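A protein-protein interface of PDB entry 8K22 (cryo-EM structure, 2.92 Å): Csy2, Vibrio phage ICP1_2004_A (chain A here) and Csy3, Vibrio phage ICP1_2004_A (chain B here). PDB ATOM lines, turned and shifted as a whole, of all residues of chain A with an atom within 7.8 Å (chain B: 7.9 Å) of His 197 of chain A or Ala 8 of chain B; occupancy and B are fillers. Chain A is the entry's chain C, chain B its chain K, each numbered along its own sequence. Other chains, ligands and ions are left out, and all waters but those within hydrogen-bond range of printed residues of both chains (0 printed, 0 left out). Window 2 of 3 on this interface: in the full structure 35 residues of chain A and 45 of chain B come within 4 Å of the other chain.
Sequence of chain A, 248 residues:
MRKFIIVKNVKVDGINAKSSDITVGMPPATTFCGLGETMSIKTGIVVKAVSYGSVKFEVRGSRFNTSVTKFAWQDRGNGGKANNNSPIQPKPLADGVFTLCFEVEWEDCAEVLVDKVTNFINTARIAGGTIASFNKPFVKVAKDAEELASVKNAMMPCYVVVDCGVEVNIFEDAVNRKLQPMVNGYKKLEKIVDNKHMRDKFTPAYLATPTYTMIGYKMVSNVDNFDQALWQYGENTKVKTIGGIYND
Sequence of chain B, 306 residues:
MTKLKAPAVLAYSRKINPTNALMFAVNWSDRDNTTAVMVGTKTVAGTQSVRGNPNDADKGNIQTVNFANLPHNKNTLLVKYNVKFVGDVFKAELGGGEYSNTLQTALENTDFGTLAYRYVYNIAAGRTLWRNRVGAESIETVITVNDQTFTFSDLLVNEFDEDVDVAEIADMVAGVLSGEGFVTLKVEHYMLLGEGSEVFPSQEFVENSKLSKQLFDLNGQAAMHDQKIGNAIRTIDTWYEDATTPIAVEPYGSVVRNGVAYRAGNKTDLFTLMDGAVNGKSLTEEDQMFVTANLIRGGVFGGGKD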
ATOM      1  N   ASP A  75      27.066  -4.492  -7.117  1.00  0.00           N
ATOM      2  CA  ASP A  75      27.830  -4.393  -5.887  1.00  0.00           C
ATOM      3  C   ASP A  75      27.497  -3.091  -5.167  1.00  0.00           C
ATOM      4  O   ASP A  75      26.927  -2.162  -5.740  1.00  0.00           O
ATOM      5  CB  ASP A  75      29.326  -4.480  -6.172  1.00  0.00           C
ATOM      6  CG  ASP A  75      29.784  -5.896  -6.443  1.00  0.00           C
ATOM      7  OD1 ASP A  75      29.000  -6.834  -6.185  1.00  0.00           O
ATOM      8  OD2 ASP A  75      30.927  -6.074  -6.915  1.00  0.00           O
ATOM      9  N   ARG A  76      27.855  -3.035  -3.892  1.00  0.00           N
ATOM     10  CA  ARG A  76      27.546  -1.893  -3.046  1.00  0.00           C
ATOM     11  C   ARG A  76      28.750  -0.970  -2.957  1.00  0.00           C
ATOM     12  O   ARG A  76      29.882  -1.423  -2.769  1.00  0.00           O
ATOM     13  CB  ARG A  76      27.133  -2.354  -1.647  1.00  0.00           C
ATOM     14  CG  ARG A  76      26.759  -1.235  -0.688  1.00  0.00           C
ATOM     15  CD  ARG A  76      26.470  -1.780   0.700  1.00  0.00           C
ATOM     16  NE  ARG A  76      25.921  -3.129   0.637  1.00  0.00           N
ATOM     17  CZ  ARG A  76      24.648  -3.427   0.847  1.00  0.00           C
ATOM     18  NH1 ARG A  76      23.765  -2.500   1.176  1.00  0.00           N
ATOM     19  NH2 ARG A  76      24.251  -4.691   0.728  1.00  0.00           N
ATOM     20  N   ASP A 194      36.789 -18.763   7.957  1.00  0.00           N
ATOM     21  CA  ASP A 194      35.816 -17.675   8.030  1.00  0.00           C
ATOM     22  C   ASP A 194      34.502 -18.158   7.429  1.00  0.00           C
ATOM     23  O   ASP A 194      34.366 -18.249   6.205  1.00  0.00           O
ATOM     24  CB  ASP A 194      36.329 -16.432   7.311  1.00  0.00           C
ATOM     25  CG  ASP A 194      35.465 -15.215   7.568  1.00  0.00           C
ATOM     26  OD1 ASP A 194      35.567 -14.632   8.668  1.00  0.00           O
ATOM     27  OD2 ASP A 194      34.678 -14.844   6.673  1.00  0.00           O
ATOM     28  N   ASN A 195      33.534 -18.456   8.289  1.00  0.00           N
ATOM     29  CA  ASN A 195      32.220 -18.909   7.862  1.00  0.00           C
ATOM     30  C   ASN A 195      31.180 -17.797   7.884  1.00  0.00           C
ATOM     31  O   ASN A 195      29.984 -18.081   7.764  1.00  0.00           O
ATOM     32  CB  ASN A 195      31.753 -20.072   8.739  1.00  0.00           C
ATOM     33  CG  ASN A 195      32.006 -19.825  10.210  1.00  0.00           C
ATOM     34  OD1 ASN A 195      32.634 -18.835  10.585  1.00  0.00           O
ATOM     35  ND2 ASN A 195      31.518 -20.726  11.055  1.00  0.00           N
ATOM     36  N   LYS A 196      31.607 -16.545   8.048  1.00  0.00           N
ATOM     37  CA  LYS A 196      30.661 -15.437   8.125  1.00  0.00           C
ATOM     38  C   LYS A 196      30.053 -15.133   6.761  1.00  0.00           C
ATOM     39  O   LYS A 196      28.847 -14.876   6.656  1.00  0.00           O
ATOM     40  CB  LYS A 196      31.360 -14.206   8.708  1.00  0.00           C
ATOM     41  CG  LYS A 196      30.592 -12.892   8.570  1.00  0.00           C
ATOM     42  CD  LYS A 196      30.804 -11.894   9.730  1.00  0.00           C
ATOM     43  CE  LYS A 196      32.130 -12.013  10.502  1.00  0.00           C
ATOM     44  NZ  LYS A 196      33.377 -11.821   9.690  1.00  0.00           N
ATOM     45  N   HIS A 197      30.859 -15.194   5.704  1.00  0.00           N
ATOM     46  CA  HIS A 197      30.416 -14.846   4.362  1.00  0.00           C
ATOM     47  C   HIS A 197      29.948 -16.053   3.560  1.00  0.00           C
ATOM     48  O   HIS A 197      30.102 -16.065   2.335  1.00  0.00           O
ATOM     49  CB  HIS A 197      31.537 -14.131   3.607  1.00  0.00           C
ATOM     50  CG  HIS A 197      32.170 -13.015   4.375  1.00  0.00           C
ATOM     51  ND1 HIS A 197      31.436 -12.005   4.959  1.00  0.00           N
ATOM     52  CD2 HIS A 197      33.467 -12.744   4.647  1.00  0.00           C
ATOM     53  CE1 HIS A 197      32.256 -11.163   5.563  1.00  0.00           C
ATOM     54  NE2 HIS A 197      33.493 -11.589   5.389  1.00  0.00           N
ATOM     55  N   MET A 198      29.390 -17.066   4.213  1.00  0.00           N
ATOM     56  CA  MET A 198      28.983 -18.287   3.538  1.00  0.00           C
ATOM     57  C   MET A 198      27.491 -18.550   3.676  1.00  0.00           C
ATOM     58  O   MET A 198      26.757 -17.834   4.361  1.00  0.00           O
ATOM     59  CB  MET A 198      29.773 -19.483   4.050  1.00  0.00           C
ATOM     60  CG  MET A 198      31.225 -19.306   3.860  1.00  0.00           C
ATOM     61  SD  MET A 198      31.828 -20.778   3.065  1.00  0.00           S
ATOM     62  CE  MET A 198      33.428 -20.182   2.631  1.00  0.00           C
ATOM     63  N   ARG A 199      27.058 -19.603   2.978  1.00  0.00           N
ATOM     64  CA  ARG A 199      25.658 -19.999   2.985  1.00  0.00           C
ATOM     65  C   ARG A 199      25.243 -20.538   4.348  1.00  0.00           C
ATOM     66  O   ARG A 199      24.228 -20.109   4.908  1.00  0.00           O
ATOM     67  CB  ARG A 199      25.430 -21.033   1.887  1.00  0.00           C
ATOM     68  CG  ARG A 199      26.041 -20.620   0.553  1.00  0.00           C
ATOM     69  CD  ARG A 199      26.012 -21.732  -0.478  1.00  0.00           C
ATOM     70  NE  ARG A 199      24.724 -21.823  -1.151  1.00  0.00           N
ATOM     71  CZ  ARG A 199      24.470 -22.631  -2.171  1.00  0.00           C
ATOM     72  NH1 ARG A 199      25.403 -23.416  -2.679  1.00  0.00           N
ATOM     73  NH2 ARG A 199      23.248 -22.650  -2.694  1.00  0.00           N
ATOM     74  N   ASP A 200      26.008 -21.483   4.895  1.00  0.00           N
ATOM     75  CA  ASP A 200      25.845 -21.940   6.267  1.00  0.00           C
ATOM     76  C   ASP A 200      27.072 -21.565   7.083  1.00  0.00           C
ATOM     77  O   ASP A 200      28.186 -21.483   6.560  1.00  0.00           O
ATOM     78  CB  ASP A 200      25.646 -23.459   6.383  1.00  0.00           C
ATOM     79  CG  ASP A 200      24.653 -24.019   5.388  1.00  0.00           C
ATOM     80  OD1 ASP A 200      23.947 -23.248   4.713  1.00  0.00           O
ATOM     81  OD2 ASP A 200      24.549 -25.260   5.305  1.00  0.00           O
ATOM     82  N   LYS A 201      26.855 -21.343   8.377  1.00  0.00           N
ATOM     83  CA  LYS A 201      27.941 -21.115   9.316  1.00  0.00           C
ATOM     84  C   LYS A 201      28.440 -22.397   9.966  1.00  0.00           C
ATOM     85  O   LYS A 201      29.540 -22.401  10.528  1.00  0.00           O
ATOM     86  CB  LYS A 201      27.494 -20.140  10.409  1.00  0.00           C
ATOM     87  CG  LYS A 201      26.536 -19.055   9.923  1.00  0.00           C
ATOM     88  CD  LYS A 201      26.412 -17.877  10.899  1.00  0.00           C
ATOM     89  CE  LYS A 201      27.738 -17.435  11.522  1.00  0.00           C
ATOM     90  NZ  LYS A 201      28.797 -17.096  10.522  1.00  0.00           N
ATOM     91  N   LYS B   5      24.155  -3.594  10.012  1.00  0.00           N
ATOM     92  CA  LYS B   5      24.873  -3.478   8.754  1.00  0.00           C
ATOM     93  C   LYS B   5      24.515  -4.618   7.808  1.00  0.00           C
ATOM     94  O   LYS B   5      24.088  -5.697   8.225  1.00  0.00           O
ATOM     95  CB  LYS B   5      26.387  -3.459   8.997  1.00  0.00           C
ATOM     96  CG  LYS B   5      26.983  -2.140   9.548  1.00  0.00           C
ATOM     97  CD  LYS B   5      26.897  -0.849   8.680  1.00  0.00           C
ATOM     98  CE  LYS B   5      26.928  -1.038   7.154  1.00  0.00           C
ATOM     99  NZ  LYS B   5      28.275  -1.441   6.663  1.00  0.00           N
ATOM    100  N   ALA B   6      24.697  -4.359   6.518  1.00  0.00           N
ATOM    101  CA  ALA B   6      24.403  -5.342   5.494  1.00  0.00           C
ATOM    102  C   ALA B   6      25.490  -6.416   5.457  1.00  0.00           C
ATOM    103  O   ALA B   6      26.628  -6.165   5.859  1.00  0.00           O
ATOM    104  CB  ALA B   6      24.294  -4.656   4.137  1.00  0.00           C
ATOM    105  N   PRO B   7      25.161  -7.627   5.003  1.00  0.00           N
ATOM    106  CA  PRO B   7      26.205  -8.630   4.789  1.00  0.00           C
ATOM    107  C   PRO B   7      27.099  -8.234   3.632  1.00  0.00           C
ATOM    108  O   PRO B   7      26.706  -7.471   2.747  1.00  0.00           O
ATOM    109  CB  PRO B   7      25.421  -9.907   4.469  1.00  0.00           C
ATOM    110  CG  PRO B   7      24.053  -9.654   4.958  1.00  0.00           C
ATOM    111  CD  PRO B   7      23.826  -8.198   4.775  1.00  0.00           C
ATOM    112  N   ALA B   8      28.326  -8.752   3.658  1.00  0.00           N
ATOM    113  CA  ALA B   8      29.300  -8.388   2.639  1.00  0.00           C
ATOM    114  C   ALA B   8      28.945  -8.969   1.279  1.00  0.00           C
ATOM    115  O   ALA B   8      29.257  -8.363   0.250  1.00  0.00           O
ATOM    116  CB  ALA B   8      30.694  -8.847   3.060  1.00  0.00           C
ATOM    117  N   VAL B   9      28.306 -10.133   1.252  1.00  0.00           N
ATOM    118  CA  VAL B   9      28.094 -10.855   0.004  1.00  0.00           C
ATOM    119  C   VAL B   9      26.628 -11.298  -0.094  1.00  0.00           C
ATOM    120  O   VAL B   9      26.309 -12.349  -0.662  1.00  0.00           O
ATOM    121  CB  VAL B   9      29.146 -11.991  -0.097  1.00  0.00           C
ATOM    122  CG1 VAL B   9      28.944 -13.115   0.953  1.00  0.00           C
ATOM    123  CG2 VAL B   9      29.367 -12.489  -1.548  1.00  0.00           C
ATOM    124  N   LEU B  10      25.727 -10.478   0.462  1.00  0.00           N
ATOM    125  CA  LEU B  10      24.287 -10.755   0.460  1.00  0.00           C
ATOM    126  C   LEU B  10      23.738 -10.912  -0.956  1.00  0.00           C
ATOM    127  O   LEU B  10      23.965 -10.067  -1.820  1.00  0.00           O
ATOM    128  CB  LEU B  10      23.548  -9.623   1.177  1.00  0.00           C
ATOM    129  CG  LEU B  10      22.043  -9.405   0.965  1.00  0.00           C
ATOM    130  CD1 LEU B  10      21.198 -10.579   1.428  1.00  0.00           C
ATOM    131  CD2 LEU B  10      21.592  -8.129   1.651  1.00  0.00           C
ATOM    132  N   ALA B  11      23.011 -12.003  -1.187  1.00  0.00           N
ATOM    133  CA  ALA B  11      22.593 -12.371  -2.530  1.00  0.00           C
ATOM    134  C   ALA B  11      21.137 -12.800  -2.536  1.00  0.00           C
ATOM    135  O   ALA B  11      20.627 -13.343  -1.554  1.00  0.00           O
ATOM    136  CB  ALA B  11      23.455 -13.502  -3.096  1.00  0.00           C
ATOM    137  N   LEU B  94      22.635 -16.372   0.222  1.00  0.00           N
ATOM    138  CA  LEU B  94      23.969 -16.131   0.747  1.00  0.00           C
ATOM    139  C   LEU B  94      23.993 -15.171   1.922  1.00  0.00           C
ATOM    140  O   LEU B  94      24.835 -15.328   2.808  1.00  0.00           O
ATOM    141  CB  LEU B  94      24.889 -15.596  -0.356  1.00  0.00           C
ATOM    142  CG  LEU B  94      26.393 -15.664  -0.093  1.00  0.00           C
ATOM    143  CD1 LEU B  94      26.791 -16.972   0.552  1.00  0.00           C
ATOM    144  CD2 LEU B  94      27.142 -15.479  -1.382  1.00  0.00           C
ATOM    145  N   GLY B  95      23.098 -14.191   1.960  1.00  0.00           N
ATOM    146  CA  GLY B  95      23.025 -13.312   3.104  1.00  0.00           C
ATOM    147  C   GLY B  95      22.466 -14.007   4.326  1.00  0.00           C
ATOM    148  O   GLY B  95      21.705 -14.971   4.243  1.00  0.00           O
ATOM    149  N   GLY B  96      22.857 -13.497   5.487  1.00  0.00           N
ATOM    150  CA  GLY B  96      22.498 -14.110   6.745  1.00  0.00           C
ATOM    151  C   GLY B  96      21.039 -13.896   7.100  1.00  0.00           C
ATOM    152  O   GLY B  96      20.291 -13.176   6.442  1.00  0.00           O
ATOM    153  N   VAL B 300      23.885 -10.305  -6.355  1.00  0.00           N
ATOM    154  CA  VAL B 300      24.783 -10.269  -5.212  1.00  0.00           C
ATOM    155  C   VAL B 300      25.186  -8.823  -4.968  1.00  0.00           C
ATOM    156  O   VAL B 300      25.208  -7.995  -5.884  1.00  0.00           O
ATOM    157  CB  VAL B 300      25.992 -11.203  -5.432  1.00  0.00           C
ATOM    158  CG1 VAL B 300      25.512 -12.497  -6.021  1.00  0.00           C
ATOM    159  CG2 VAL B 300      27.050 -10.585  -6.331  1.00  0.00           C
ATOM    160  N   PHE B 301      25.429  -8.489  -3.708  1.00  0.00           N
ATOM    161  CA  PHE B 301      25.619  -7.102  -3.296  1.00  0.00           C
ATOM    162  C   PHE B 301      26.915  -7.030  -2.496  1.00  0.00           C
ATOM    163  O   PHE B 301      26.934  -7.336  -1.301  1.00  0.00           O
ATOM    164  CB  PHE B 301      24.418  -6.611  -2.492  1.00  0.00           C
ATOM    165  CG  PHE B 301      23.085  -6.893  -3.149  1.00  0.00           C
ATOM    166  CD1 PHE B 301      22.819  -6.457  -4.437  1.00  0.00           C
ATOM    167  CD2 PHE B 301      22.095  -7.582  -2.469  1.00  0.00           C
ATOM    168  CE1 PHE B 301      21.603  -6.720  -5.042  1.00  0.00           C
ATOM    169  CE2 PHE B 301      20.873  -7.844  -3.068  1.00  0.00           C
ATOM    170  CZ  PHE B 301      20.629  -7.408  -4.354  1.00  0.00           C
ATOM    171  N   GLY B 302      27.994  -6.628  -3.159  1.00  0.00           N
ATOM    172  CA  GLY B 302      29.304  -6.618  -2.541  1.00  0.00           C
ATOM    173  C   GLY B 302      29.573  -5.399  -1.685  1.00  0.00           C
ATOM    174  O   GLY B 302      29.802  -4.305  -2.206  1.00  0.00           O
ATOM    175  N   GLY B 303      29.559  -5.578  -0.371  1.00  0.00           N
ATOM    176  CA  GLY B 303      29.815  -4.490   0.551  1.00  0.00           C
ATOM    177  C   GLY B 303      29.312  -4.773   1.950  1.00  0.00           C
ATOM    178  O   GLY B 303      30.095  -5.061   2.853  1.00  0.00           O
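The backbone NH (N) of Gly 303 of chain B sits at hydrogen-bond distance from the backbone carbonyl oxygen (O) of Ala 8 of chain B (2.9 Å).
N of Phe 301 of chain B sits at hydrogen-bond distance from O of Leu 10 of chain B.
Among the printed residues, merely in contact across the chains: Asp 75 of chain A with Val 300 of chain B, Arg 76 of chain A with Ala 6 of chain B, Arg 76 of chain A with Phe 301 of chain B, Arg 76 of chain A with Gly 303 of chain B, His 197 of chain A with Ala 8 of chain B, His 197 of chain A with Val 9 of chain B, His 197 of chain A with Leu 94 of chain B, Met 198 of chain A with Leu 94 of chain B and Arg 199 of chain A with Leu 94 of chain B.
Printed residues of chain B within 4 Å of Asp 75 of chain A: Val 300 (3.98 Å) and Gly 302 (3.2 Å).
Printed residues of chain B within 4 Å of Arg 76 of chain A: Ala 6, Phe 301, Gly 302 and Gly 303.
Of chain B, only Ala 8 (3.8 Å), Val 9 (3.5 Å) and Leu 94 (3.9 Å) come within 4 Å of His 197 of chain A.
Printed residues of chain B within 4 Å of Arg 199 of chain A: Leu 94 (3.6 Å).
Asp 200 of chain A touches none of the printed residues of chain B.
Of chain A, only His 197 (3.8 Å) comes within 4 Å of Ala 8 of chain B.
Ala 11 of chain B touches none of the printed residues of chain A.
Of the printed residues of chain A, Gly 302 of chain B touches Asp 75 and Arg 76.
Printed residues of chain A within 4 Å of Gly 303 of chain B: Arg 76 (3.99 Å).
The nearest residue of chain B that does not touch His 197 of chain A is Pro 7 of chain B (5.9 Å).
The nearest residue of chain A that does not touch Ala 8 of chain B is Arg 76 of chain A (6.2 Å).
The nearest printed residue of chain B that does not touch Arg 76 of chain A is Pro 7 of chain B (4.2 Å).
Of the 10 printed residues of chain A, 5 touch a printed residue of chain B.
Hydrophobic or aromatic side chains of chain A within 4 Å of the printed part of chain B: His 197.
OD1 of Asp 75 of chain A is in hydrogen-bond range of N of Gly 302 of chain B, at 3.2 Å.
The backbone carbonyl oxygen (O) of Gly 302 of chain B lies within hydrogen-bond range of the backbone NH (N) of Arg 76 of chain A (2.9 Å).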
